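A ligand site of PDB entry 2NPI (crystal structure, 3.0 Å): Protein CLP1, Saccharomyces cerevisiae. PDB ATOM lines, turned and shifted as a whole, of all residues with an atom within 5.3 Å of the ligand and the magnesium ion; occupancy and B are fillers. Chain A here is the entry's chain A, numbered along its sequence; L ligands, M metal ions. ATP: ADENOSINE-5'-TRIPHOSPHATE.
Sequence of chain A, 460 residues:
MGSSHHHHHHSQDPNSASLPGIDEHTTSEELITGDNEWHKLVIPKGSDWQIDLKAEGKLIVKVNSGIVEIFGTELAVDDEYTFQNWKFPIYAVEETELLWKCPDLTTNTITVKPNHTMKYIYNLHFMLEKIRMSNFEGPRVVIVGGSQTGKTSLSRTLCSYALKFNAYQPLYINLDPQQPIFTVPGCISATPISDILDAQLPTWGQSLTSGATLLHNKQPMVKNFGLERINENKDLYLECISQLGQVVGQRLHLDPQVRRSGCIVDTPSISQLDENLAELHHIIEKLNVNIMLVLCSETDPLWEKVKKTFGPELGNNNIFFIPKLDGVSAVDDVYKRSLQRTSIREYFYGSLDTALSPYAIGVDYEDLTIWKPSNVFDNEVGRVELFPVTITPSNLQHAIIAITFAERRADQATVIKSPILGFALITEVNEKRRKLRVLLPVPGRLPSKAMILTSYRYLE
The magnesium ion is bound by O2G of the ligand (2.1 Å), O1B of the ligand (2.2 Å) and OG1 of Thr 152 (2.4 Å).
The side-chain hydroxyl (OG1) of Thr 152 lies close to the side-chain carboxylate (OD2) of Asp 266 (2.8 Å). N of Lys 87 lies within hydrogen-bond range of OH of Tyr 335 (3.0 Å). The backbone NH (N) of Val 331 lies close to the side-chain amide nitrogen (NE2) of Gln 148 (3.1 Å). The side-chain carboxylate (OD2) of Asp 48 lies within hydrogen-bond range of the side-chain amide nitrogen (ND2) of Asn 115, at 2.8 Å. N of Ile 51 lies within hydrogen-bond range of O of Phe 88 (2.9 Å).
The backbone carbonyl oxygen of Gly 327 sits close to a nitrogen (N3) of the ligand, 3.0 Å away. Gln 50 touches the ligand. Phe 71 touches the ligand. Phe 88 touches the ligand (CA to O2', 3.9 Å). Pro 89 touches the ligand (CB to N1, 3.3 Å). Asn 115 touches the ligand (ND2 to N6, 3.9 Å). OG of Ser 147 touches O3G of the ligand, at 3.7 Å. Asp 176 touches the ligand (OD2 to O2G, 3.9 Å). Val 328 touches the ligand (CG1 to O5', 3.6 Å). N of Ser 329 touches O4' of the ligand, 3.5 Å away. Val 331 touches the ligand. Tyr 335 touches the ligand. Within 4 Å of the ligand: Asp 48, Gln 50, Phe 71, Lys 87, Phe 88, Pro 89, Asn 115, Ser 147, Gln 148, Thr 149, Gly 150, Lys 151, Thr 152, Ser 153, Asp 176, Asp 326, Gly 327, Val 328, Ser 329, Val 331 and Tyr 335.
N of Thr 152 lies close to O1B of the ligand (3.2 Å). The backbone carbonyl oxygen (O) of Lys 87 lies within hydrogen-bond range of an oxygen (O2') of the ligand (2.5 Å). The backbone NH of Lys 151 is in hydrogen-bond range of an oxygen (O2B) of the ligand (2.6 Å). The side-chain amino group of Lys 151 is in salt-bridge range of an oxygen (O3G) of the ligand, at 3.6 Å. O2B of the ligand sits at hydrogen-bond distance from N of Gly 150 (2.6 Å). The backbone NH (N) of Ser 153 sits at hydrogen-bond distance from an oxygen (O2A) of the ligand. The side-chain hydroxyl of Ser 153 is in hydrogen-bond range of an oxygen (O2A) of the ligand (2.9 Å). The backbone carbonyl oxygen (O) of Asp 326 is in hydrogen-bond range of a nitrogen (N6) of the ligand, 3.0 Å away. The backbone NH (N) of Gln 148 sits at hydrogen-bond distance from an oxygen (O3B) of the ligand (3.2 Å). O3G of the ligand lies close to OE1 of Gln 148 (3.1 Å). The backbone NH of Thr 149 is in hydrogen-bond range of an oxygen (O2B) of the ligand. The side-chain carboxylate (OD2) of Asp 48 sits at hydrogen-bond distance from a nitrogen (N6) of the ligand.
Asp 176 touches the magnesium ion (OD2 to MG, 3.95 Å). OE1 of Gln 179 touches the magnesium ion, at 3.7 Å.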
ATOM      1  N   ASP A  48       6.427 -17.348   7.630  1.00  0.00           N
ATOM      2  CA  ASP A  48       7.747 -16.734   7.558  1.00  0.00           C
ATOM      3  C   ASP A  48       7.652 -15.224   7.731  1.00  0.00           C
ATOM      4  O   ASP A  48       6.681 -14.599   7.301  1.00  0.00           O
ATOM      5  CB  ASP A  48       8.408 -17.021   6.215  1.00  0.00           C
ATOM      6  CG  ASP A  48       9.038 -18.404   6.151  1.00  0.00           C
ATOM      7  OD1 ASP A  48       9.792 -18.761   7.085  1.00  0.00           O
ATOM      8  OD2 ASP A  48       8.799 -19.110   5.147  1.00  0.00           O
ATOM      9  N   GLN A  50      10.319 -13.169   6.501  1.00  0.00           N
ATOM     10  CA  GLN A  50      10.874 -12.709   5.210  1.00  0.00           C
ATOM     11  C   GLN A  50      11.401 -11.284   5.320  1.00  0.00           C
ATOM     12  O   GLN A  50      10.630 -10.317   5.303  1.00  0.00           O
ATOM     13  CB  GLN A  50       9.855 -12.804   4.062  1.00  0.00           C
ATOM     14  CG  GLN A  50       9.378 -14.211   3.731  1.00  0.00           C
ATOM     15  CD  GLN A  50       8.559 -14.272   2.440  1.00  0.00           C
ATOM     16  OE1 GLN A  50       8.126 -15.351   2.033  1.00  0.00           O
ATOM     17  NE2 GLN A  50       8.363 -13.126   1.805  1.00  0.00           N
ATOM     18  N   ILE A  51      12.724 -11.157   5.421  1.00  0.00           N
ATOM     19  CA  ILE A  51      13.359  -9.889   5.742  1.00  0.00           C
ATOM     20  C   ILE A  51      14.422  -9.558   4.695  1.00  0.00           C
ATOM     21  O   ILE A  51      15.186 -10.420   4.295  1.00  0.00           O
ATOM     22  CB  ILE A  51      13.998  -9.947   7.146  1.00  0.00           C
ATOM     23  CG1 ILE A  51      12.938 -10.311   8.195  1.00  0.00           C
ATOM     24  CG2 ILE A  51      14.658  -8.621   7.512  1.00  0.00           C
ATOM     25  CD1 ILE A  51      13.494 -10.861   9.481  1.00  0.00           C
ATOM     26  N   PHE A  71      16.365 -20.921   9.071  1.00  0.00           N
ATOM     27  CA  PHE A  71      16.845 -22.102   8.324  1.00  0.00           C
ATOM     28  C   PHE A  71      17.142 -23.283   9.260  1.00  0.00           C
ATOM     29  O   PHE A  71      18.160 -23.966   9.112  1.00  0.00           O
ATOM     30  CB  PHE A  71      18.072 -21.775   7.473  1.00  0.00           C
ATOM     31  CG  PHE A  71      17.914 -20.589   6.550  1.00  0.00           C
ATOM     32  CD1 PHE A  71      18.643 -19.429   6.744  1.00  0.00           C
ATOM     33  CD2 PHE A  71      17.041 -20.655   5.463  1.00  0.00           C
ATOM     34  CE1 PHE A  71      18.517 -18.336   5.893  1.00  0.00           C
ATOM     35  CE2 PHE A  71      16.901 -19.557   4.612  1.00  0.00           C
ATOM     36  CZ  PHE A  71      17.643 -18.406   4.825  1.00  0.00           C
ATOM     37  N   TRP A  86      21.649  -8.914   5.055  1.00  0.00           N
ATOM     38  CA  TRP A  86      21.245 -10.131   4.338  1.00  0.00           C
ATOM     39  C   TRP A  86      19.749 -10.400   4.365  1.00  0.00           C
ATOM     40  O   TRP A  86      19.050 -10.016   5.310  1.00  0.00           O
ATOM     41  CB  TRP A  86      22.046 -11.368   4.805  1.00  0.00           C
ATOM     42  CG  TRP A  86      21.688 -11.925   6.168  1.00  0.00           C
ATOM     43  CD1 TRP A  86      21.679 -11.251   7.357  1.00  0.00           C
ATOM     44  CD2 TRP A  86      21.333 -13.279   6.478  1.00  0.00           C
ATOM     45  NE1 TRP A  86      21.320 -12.099   8.383  1.00  0.00           N
ATOM     46  CE2 TRP A  86      21.112 -13.345   7.878  1.00  0.00           C
ATOM     47  CE3 TRP A  86      21.187 -14.448   5.715  1.00  0.00           C
ATOM     48  CZ2 TRP A  86      20.733 -14.528   8.517  1.00  0.00           C
ATOM     49  CZ3 TRP A  86      20.818 -15.627   6.354  1.00  0.00           C
ATOM     50  CH2 TRP A  86      20.603 -15.653   7.743  1.00  0.00           C
ATOM     51  N   LYS A  87      19.253 -11.055   3.318  1.00  0.00           N
ATOM     52  CA  LYS A  87      17.850 -11.458   3.233  1.00  0.00           C
ATOM     53  C   LYS A  87      17.654 -12.834   3.848  1.00  0.00           C
ATOM     54  O   LYS A  87      18.396 -13.771   3.533  1.00  0.00           O
ATOM     55  CB  LYS A  87      17.363 -11.409   1.778  1.00  0.00           C
ATOM     56  CG  LYS A  87      15.978 -12.001   1.576  1.00  0.00           C
ATOM     57  CD  LYS A  87      15.110 -11.133   0.680  1.00  0.00           C
ATOM     58  CE  LYS A  87      13.633 -11.466   0.878  1.00  0.00           C
ATOM     59  NZ  LYS A  87      12.758 -10.542   0.119  1.00  0.00           N
ATOM     60  N   PHE A  88      16.656 -12.962   4.729  1.00  0.00           N
ATOM     61  CA  PHE A  88      16.431 -14.203   5.479  1.00  0.00           C
ATOM     62  C   PHE A  88      15.015 -14.296   6.064  1.00  0.00           C
ATOM     63  O   PHE A  88      14.450 -13.290   6.480  1.00  0.00           O
ATOM     64  CB  PHE A  88      17.465 -14.345   6.611  1.00  0.00           C
ATOM     65  CG  PHE A  88      17.311 -13.337   7.723  1.00  0.00           C
ATOM     66  CD1 PHE A  88      16.712 -13.695   8.924  1.00  0.00           C
ATOM     67  CD2 PHE A  88      17.753 -12.021   7.559  1.00  0.00           C
ATOM     68  CE1 PHE A  88      16.568 -12.767   9.965  1.00  0.00           C
ATOM     69  CE2 PHE A  88      17.596 -11.086   8.592  1.00  0.00           C
ATOM     70  CZ  PHE A  88      17.005 -11.462   9.789  1.00  0.00           C
ATOM     71  N   PRO A  89      14.439 -15.513   6.074  1.00  0.00           N
ATOM     72  CA  PRO A  89      13.184 -15.781   6.763  1.00  0.00           C
ATOM     73  C   PRO A  89      13.346 -16.127   8.236  1.00  0.00           C
ATOM     74  O   PRO A  89      14.271 -16.860   8.609  1.00  0.00           O
ATOM     75  CB  PRO A  89      12.637 -16.989   6.016  1.00  0.00           C
ATOM     76  CG  PRO A  89      13.846 -17.736   5.598  1.00  0.00           C
ATOM     77  CD  PRO A  89      14.923 -16.709   5.354  1.00  0.00           C
ATOM     78  N   ASN A 115       4.236 -20.194   5.019  1.00  0.00           N
ATOM     79  CA  ASN A 115       5.055 -21.142   4.271  1.00  0.00           C
ATOM     80  C   ASN A 115       4.361 -22.491   4.186  1.00  0.00           C
ATOM     81  O   ASN A 115       3.902 -23.025   5.204  1.00  0.00           O
ATOM     82  CB  ASN A 115       6.420 -21.294   4.933  1.00  0.00           C
ATOM     83  CG  ASN A 115       7.395 -22.091   4.079  1.00  0.00           C
ATOM     84  OD1 ASN A 115       7.171 -23.257   3.787  1.00  0.00           O
ATOM     85  ND2 ASN A 115       8.489 -21.449   3.692  1.00  0.00           N
ATOM     86  N   GLY A 146      17.868 -25.127 -10.146  1.00  0.00           N
ATOM     87  CA  GLY A 146      18.021 -23.893 -10.909  1.00  0.00           C
ATOM     88  C   GLY A 146      18.533 -22.735 -10.061  1.00  0.00           C
ATOM     89  O   GLY A 146      18.778 -22.891  -8.861  1.00  0.00           O
ATOM     90  N   SER A 147      18.696 -21.583 -10.699  1.00  0.00           N
ATOM     91  CA  SER A 147      19.170 -20.395 -10.009  1.00  0.00           C
ATOM     92  C   SER A 147      18.120 -19.926  -8.997  1.00  0.00           C
ATOM     93  O   SER A 147      16.944 -19.819  -9.338  1.00  0.00           O
ATOM     94  CB  SER A 147      19.505 -19.294 -11.006  1.00  0.00           C
ATOM     95  OG  SER A 147      20.638 -18.552 -10.587  1.00  0.00           O
ATOM     96  N   GLN A 148      18.569 -19.671  -7.768  1.00  0.00           N
ATOM     97  CA  GLN A 148      17.680 -19.299  -6.654  1.00  0.00           C
ATOM     98  C   GLN A 148      16.449 -20.190  -6.524  1.00  0.00           C
ATOM     99  O   GLN A 148      15.312 -19.748  -6.734  1.00  0.00           O
ATOM    100  CB  GLN A 148      17.275 -17.819  -6.719  1.00  0.00           C
ATOM    101  CG  GLN A 148      18.316 -16.845  -6.174  1.00  0.00           C
ATOM    102  CD  GLN A 148      19.338 -16.424  -7.201  1.00  0.00           C
ATOM    103  OE1 GLN A 148      20.507 -16.781  -7.104  1.00  0.00           O
ATOM    104  NE2 GLN A 148      18.909 -15.657  -8.206  1.00  0.00           N
ATOM    105  N   THR A 149      16.676 -21.456  -6.185  1.00  0.00           N
ATOM    106  CA  THR A 149      15.580 -22.401  -5.994  1.00  0.00           C
ATOM    107  C   THR A 149      15.416 -22.846  -4.539  1.00  0.00           C
ATOM    108  O   THR A 149      14.364 -23.358  -4.142  1.00  0.00           O
ATOM    109  CB  THR A 149      15.705 -23.620  -6.930  1.00  0.00           C
ATOM    110  OG1 THR A 149      14.518 -24.429  -6.821  1.00  0.00           O
ATOM    111  CG2 THR A 149      16.943 -24.460  -6.598  1.00  0.00           C
ATOM    112  N   GLY A 150      16.472 -22.641  -3.745  1.00  0.00           N
ATOM    113  CA  GLY A 150      16.452 -22.957  -2.320  1.00  0.00           C
ATOM    114  C   GLY A 150      17.532 -23.922  -1.856  1.00  0.00           C
ATOM    115  O   GLY A 150      17.545 -24.319  -0.696  1.00  0.00           O
ATOM    116  N   LYS A 151      18.433 -24.301  -2.766  1.00  0.00           N
ATOM    117  CA  LYS A 151      19.532 -25.236  -2.489  1.00  0.00           C
ATOM    118  C   LYS A 151      20.208 -24.983  -1.145  1.00  0.00           C
ATOM    119  O   LYS A 151      20.121 -25.796  -0.229  1.00  0.00           O
ATOM    120  CB  LYS A 151      20.594 -25.173  -3.590  1.00  0.00           C
ATOM    121  CG  LYS A 151      20.198 -25.813  -4.899  1.00  0.00           C
ATOM    122  CD  LYS A 151      21.134 -25.345  -6.008  1.00  0.00           C
ATOM    123  CE  LYS A 151      20.757 -23.950  -6.473  1.00  0.00           C
ATOM    124  NZ  LYS A 151      21.918 -23.220  -7.013  1.00  0.00           N
ATOM    125  N   THR A 152      20.892 -23.843  -1.049  1.00  0.00           N
ATOM    126  CA  THR A 152      21.681 -23.501   0.134  1.00  0.00           C
ATOM    127  C   THR A 152      20.797 -23.459   1.375  1.00  0.00           C
ATOM    128  O   THR A 152      21.162 -24.008   2.422  1.00  0.00           O
ATOM    129  CB  THR A 152      22.450 -22.176  -0.064  1.00  0.00           C
ATOM    130  OG1 THR A 152      23.168 -22.214  -1.307  1.00  0.00           O
ATOM    131  CG2 THR A 152      23.440 -21.935   1.077  1.00  0.00           C
ATOM    132  N   SER A 153      19.643 -22.821   1.253  1.00  0.00           N
ATOM    133  CA  SER A 153      18.705 -22.718   2.364  1.00  0.00           C
ATOM    134  C   SER A 153      18.254 -24.113   2.807  1.00  0.00           C
ATOM    135  O   SER A 153      18.179 -24.391   4.005  1.00  0.00           O
ATOM    136  CB  SER A 153      17.518 -21.851   1.968  1.00  0.00           C
ATOM    137  OG  SER A 153      17.958 -20.584   1.525  1.00  0.00           O
ATOM    138  N   LEU A 154      17.989 -24.974   1.838  1.00  0.00           N
ATOM    139  CA  LEU A 154      17.584 -26.349   2.091  1.00  0.00           C
ATOM    140  C   LEU A 154      18.725 -27.142   2.710  1.00  0.00           C
ATOM    141  O   LEU A 154      18.504 -27.946   3.615  1.00  0.00           O
ATOM    142  CB  LEU A 154      17.085 -27.005   0.797  1.00  0.00           C
ATOM    143  CG  LEU A 154      16.372 -28.371   0.749  1.00  0.00           C
ATOM    144  CD1 LEU A 154      17.330 -29.460   0.349  1.00  0.00           C
ATOM    145  CD2 LEU A 154      15.634 -28.733   2.030  1.00  0.00           C
ATOM    146  N   ASP A 176      30.045 -24.251  -4.201  1.00  0.00           N
ATOM    147  CA  ASP A 176      29.782 -23.019  -4.950  1.00  0.00           C
ATOM    148  C   ASP A 176      30.697 -21.885  -4.472  1.00  0.00           C
ATOM    149  O   ASP A 176      30.349 -21.173  -3.526  1.00  0.00           O
ATOM    150  CB  ASP A 176      28.292 -22.627  -4.858  1.00  0.00           C
ATOM    151  CG  ASP A 176      27.955 -21.345  -5.626  1.00  0.00           C
ATOM    152  OD1 ASP A 176      28.707 -20.937  -6.547  1.00  0.00           O
ATOM    153  OD2 ASP A 176      26.909 -20.746  -5.314  1.00  0.00           O
ATOM    154  N   GLN A 179      29.659 -18.480  -3.131  1.00  0.00           N
ATOM    155  CA  GLN A 179      28.945 -18.460  -1.852  1.00  0.00           C
ATOM    156  C   GLN A 179      29.885 -18.679  -0.667  1.00  0.00           C
ATOM    157  O   GLN A 179      30.379 -19.795  -0.453  1.00  0.00           O
ATOM    158  CB  GLN A 179      27.856 -19.544  -1.869  1.00  0.00           C
ATOM    159  CG  GLN A 179      26.898 -19.489  -0.687  1.00  0.00           C
ATOM    160  CD  GLN A 179      25.736 -18.567  -0.936  1.00  0.00           C
ATOM    161  OE1 GLN A 179      24.737 -18.958  -1.537  1.00  0.00           O
ATOM    162  NE2 GLN A 179      25.850 -17.323  -0.464  1.00  0.00           N
ATOM    163  N   ASP A 266      25.974 -29.238  -1.386  1.00  0.00           N
ATOM    164  CA  ASP A 266      25.311 -28.116  -2.054  1.00  0.00           C
ATOM    165  C   ASP A 266      26.085 -27.743  -3.311  1.00  0.00           C
ATOM    166  O   ASP A 266      27.312 -27.556  -3.269  1.00  0.00           O
ATOM    167  CB  ASP A 266      25.220 -26.934  -1.085  1.00  0.00           C
ATOM    168  CG  ASP A 266      24.360 -25.798  -1.618  1.00  0.00           C
ATOM    169  OD1 ASP A 266      23.683 -25.952  -2.662  1.00  0.00           O
ATOM    170  OD2 ASP A 266      24.363 -24.721  -0.982  1.00  0.00           O
ATOM    171  N   THR A 267      25.376 -27.649  -4.429  1.00  0.00           N
ATOM    172  CA  THR A 267      25.964 -27.319  -5.720  1.00  0.00           C
ATOM    173  C   THR A 267      25.529 -25.936  -6.199  1.00  0.00           C
ATOM    174  O   THR A 267      24.538 -25.391  -5.693  1.00  0.00           O
ATOM    175  CB  THR A 267      25.575 -28.344  -6.802  1.00  0.00           C
ATOM    176  OG1 THR A 267      24.150 -28.374  -6.943  1.00  0.00           O
ATOM    177  CG2 THR A 267      26.083 -29.736  -6.437  1.00  0.00           C
ATOM    178  N   PRO A 268      26.267 -25.354  -7.170  1.00  0.00           N
ATOM    179  CA  PRO A 268      25.797 -24.145  -7.835  1.00  0.00           C
ATOM    180  C   PRO A 268      24.636 -24.481  -8.754  1.00  0.00           C
ATOM    181  O   PRO A 268      24.344 -25.667  -8.948  1.00  0.00           O
ATOM    182  CB  PRO A 268      27.007 -23.709  -8.660  1.00  0.00           C
ATOM    183  CG  PRO A 268      27.714 -24.983  -8.943  1.00  0.00           C
ATOM    184  CD  PRO A 268      27.573 -25.785  -7.696  1.00  0.00           C
ATOM    185  N   SER A 269      23.971 -23.465  -9.303  1.00  0.00           N
ATOM    186  CA  SER A 269      22.857 -23.679 -10.223  1.00  0.00           C
ATOM    187  C   SER A 269      23.330 -24.307 -11.528  1.00  0.00           C
ATOM    188  O   SER A 269      24.438 -24.036 -11.982  1.00  0.00           O
ATOM    189  CB  SER A 269      22.131 -22.362 -10.496  1.00  0.00           C
ATOM    190  OG  SER A 269      22.965 -21.478 -11.230  1.00  0.00           O
ATOM    191  N   ASP A 326       8.819 -22.145  -0.848  1.00  0.00           N
ATOM    192  CA  ASP A 326       8.180 -20.848  -0.672  1.00  0.00           C
ATOM    193  C   ASP A 326       9.180 -19.817  -0.166  1.00  0.00           C
ATOM    194  O   ASP A 326      10.142 -20.158   0.527  1.00  0.00           O
ATOM    195  CB  ASP A 326       7.017 -20.955   0.324  1.00  0.00           C
ATOM    196  CG  ASP A 326       5.801 -21.661  -0.263  1.00  0.00           C
ATOM    197  OD1 ASP A 326       5.869 -22.151  -1.406  1.00  0.00           O
ATOM    198  OD2 ASP A 326       4.762 -21.725   0.447  1.00  0.00           O
ATOM    199  N   GLY A 327       8.970 -18.560  -0.528  1.00  0.00           N
ATOM    200  CA  GLY A 327       9.759 -17.449  -0.005  1.00  0.00           C
ATOM    201  C   GLY A 327      11.145 -17.254  -0.607  1.00  0.00           C
ATOM    202  O   GLY A 327      11.773 -16.224  -0.384  1.00  0.00           O
ATOM    203  N   VAL A 328      11.625 -18.252  -1.362  1.00  0.00           N
ATOM    204  CA  VAL A 328      12.935 -18.151  -1.998  1.00  0.00           C
ATOM    205  C   VAL A 328      12.911 -17.065  -3.055  1.00  0.00           C
ATOM    206  O   VAL A 328      12.319 -17.230  -4.131  1.00  0.00           O
ATOM    207  CB  VAL A 328      13.393 -19.496  -2.610  1.00  0.00           C
ATOM    208  CG1 VAL A 328      14.853 -19.424  -3.024  1.00  0.00           C
ATOM    209  CG2 VAL A 328      13.177 -20.640  -1.631  1.00  0.00           C
ATOM    210  N   SER A 329      13.553 -15.939  -2.737  1.00  0.00           N
ATOM    211  CA  SER A 329      13.556 -14.762  -3.598  1.00  0.00           C
ATOM    212  C   SER A 329      14.796 -14.713  -4.484  1.00  0.00           C
ATOM    213  O   SER A 329      15.822 -15.311  -4.159  1.00  0.00           O
ATOM    214  CB  SER A 329      13.460 -13.487  -2.751  1.00  0.00           C
ATOM    215  OG  SER A 329      14.532 -13.407  -1.822  1.00  0.00           O
ATOM    216  N   VAL A 331      18.179 -13.323  -6.243  1.00  0.00           N
ATOM    217  CA  VAL A 331      19.366 -12.664  -5.699  1.00  0.00           C
ATOM    218  C   VAL A 331      20.186 -12.073  -6.842  1.00  0.00           C
ATOM    219  O   VAL A 331      20.561 -12.773  -7.784  1.00  0.00           O
ATOM    220  CB  VAL A 331      20.223 -13.650  -4.852  1.00  0.00           C
ATOM    221  CG1 VAL A 331      21.654 -13.153  -4.682  1.00  0.00           C
ATOM    222  CG2 VAL A 331      19.587 -13.860  -3.492  1.00  0.00           C
ATOM    223  N   TYR A 335      24.167  -7.640  -4.290  1.00  0.00           N
ATOM    224  CA  TYR A 335      23.921  -8.286  -2.998  1.00  0.00           C
ATOM    225  C   TYR A 335      24.926  -9.402  -2.756  1.00  0.00           C
ATOM    226  O   TYR A 335      25.421  -9.558  -1.645  1.00  0.00           O
ATOM    227  CB  TYR A 335      22.487  -8.838  -2.934  1.00  0.00           C
ATOM    228  CG  TYR A 335      22.225  -9.729  -1.731  1.00  0.00           C
ATOM    229  CD1 TYR A 335      21.734  -9.184  -0.539  1.00  0.00           C
ATOM    230  CD2 TYR A 335      22.447 -11.108  -1.789  1.00  0.00           C
ATOM    231  CE1 TYR A 335      21.485 -10.002   0.568  1.00  0.00           C
ATOM    232  CE2 TYR A 335      22.189 -11.927  -0.692  1.00  0.00           C
ATOM    233  CZ  TYR A 335      21.716 -11.370   0.482  1.00  0.00           C
ATOM    234  OH  TYR A 335      21.467 -12.183   1.570  1.00  0.00           O
ATOM    235  N   LYS A 336      25.217 -10.160  -3.806  1.00  0.00           N
ATOM    236  CA  LYS A 336      26.123 -11.308  -3.716  1.00  0.00           C
ATOM    237  C   LYS A 336      27.563 -10.880  -3.471  1.00  0.00           C
ATOM    238  O   LYS A 336      28.277 -11.513  -2.686  1.00  0.00           O
ATOM    239  CB  LYS A 336      25.987 -12.192  -4.957  1.00  0.00           C
ATOM    240  CG  LYS A 336      26.186 -13.679  -4.691  1.00  0.00           C
ATOM    241  CD  LYS A 336      25.294 -14.553  -5.570  1.00  0.00           C
ATOM    242  CE  LYS A 336      25.749 -14.559  -7.024  1.00  0.00           C
ATOM    243  NZ  LYS A 336      24.846 -15.389  -7.872  1.00  0.00           N
HETATM  244  PG  ATP L   1      21.915 -19.989  -5.760  1.00  0.00           P
HETATM  245  O1G ATP L   1      21.886 -18.821  -4.804  1.00  0.00           O
HETATM  246  O2G ATP L   1      22.978 -21.020  -5.477  1.00  0.00           O
HETATM  247  O3G ATP L   1      21.776 -19.625  -7.218  1.00  0.00           O
HETATM  248  PB  ATP L   1      20.119 -21.161  -3.968  1.00  0.00           P
HETATM  249  O1B ATP L   1      21.361 -21.446  -3.165  1.00  0.00           O
HETATM  250  O2B ATP L   1      19.051 -22.207  -4.109  1.00  0.00           O
HETATM  251  O3B ATP L   1      20.529 -20.741  -5.466  1.00  0.00           O
HETATM  252  PA  ATP L   1      19.322 -19.620  -1.814  1.00  0.00           P
HETATM  253  O1A ATP L   1      20.616 -18.985  -1.346  1.00  0.00           O
HETATM  254  O2A ATP L   1      18.871 -20.915  -1.172  1.00  0.00           O
HETATM  255  O3A ATP L   1      19.432 -19.832  -3.394  1.00  0.00           O
HETATM  256  O5' ATP L   1      18.122 -18.552  -1.700  1.00  0.00           O
HETATM  257  C5' ATP L   1      18.255 -17.248  -2.272  1.00  0.00           C
HETATM  258  C4' ATP L   1      17.812 -16.205  -1.249  1.00  0.00           C
HETATM  259  O4' ATP L   1      16.468 -16.469  -0.848  1.00  0.00           O
HETATM  260  C3' ATP L   1      18.676 -16.239   0.010  1.00  0.00           C
HETATM  261  O3' ATP L   1      19.197 -14.943   0.274  1.00  0.00           O
HETATM  262  C2' ATP L   1      17.746 -16.691   1.112  1.00  0.00           C
HETATM  263  O2' ATP L   1      17.980 -15.982   2.333  1.00  0.00           O
HETATM  264  C1' ATP L   1      16.371 -16.371   0.572  1.00  0.00           C
HETATM  265  N9  ATP L   1      15.330 -17.279   1.102  1.00  0.00           N
HETATM  266  C8  ATP L   1      15.339 -18.625   1.070  1.00  0.00           C
HETATM  267  N7  ATP L   1      14.211 -19.131   1.632  1.00  0.00           N
HETATM  268  C5  ATP L   1      13.451 -18.096   2.022  1.00  0.00           C
HETATM  269  C6  ATP L   1      12.142 -17.920   2.672  1.00  0.00           C
HETATM  270  N6  ATP L   1      11.394 -18.985   3.045  1.00  0.00           N
HETATM  271  N1  ATP L   1      11.717 -16.652   2.906  1.00  0.00           N
HETATM  272  C2  ATP L   1      12.448 -15.576   2.546  1.00  0.00           C
HETATM  273  N3  ATP L   1      13.649 -15.666   1.945  1.00  0.00           N
HETATM  274  C4  ATP L   1      14.198 -16.878   1.664  1.00  0.00           C
HETATM  275 MG    MG M   1      23.503 -21.809  -3.611  1.00  0.00          MG
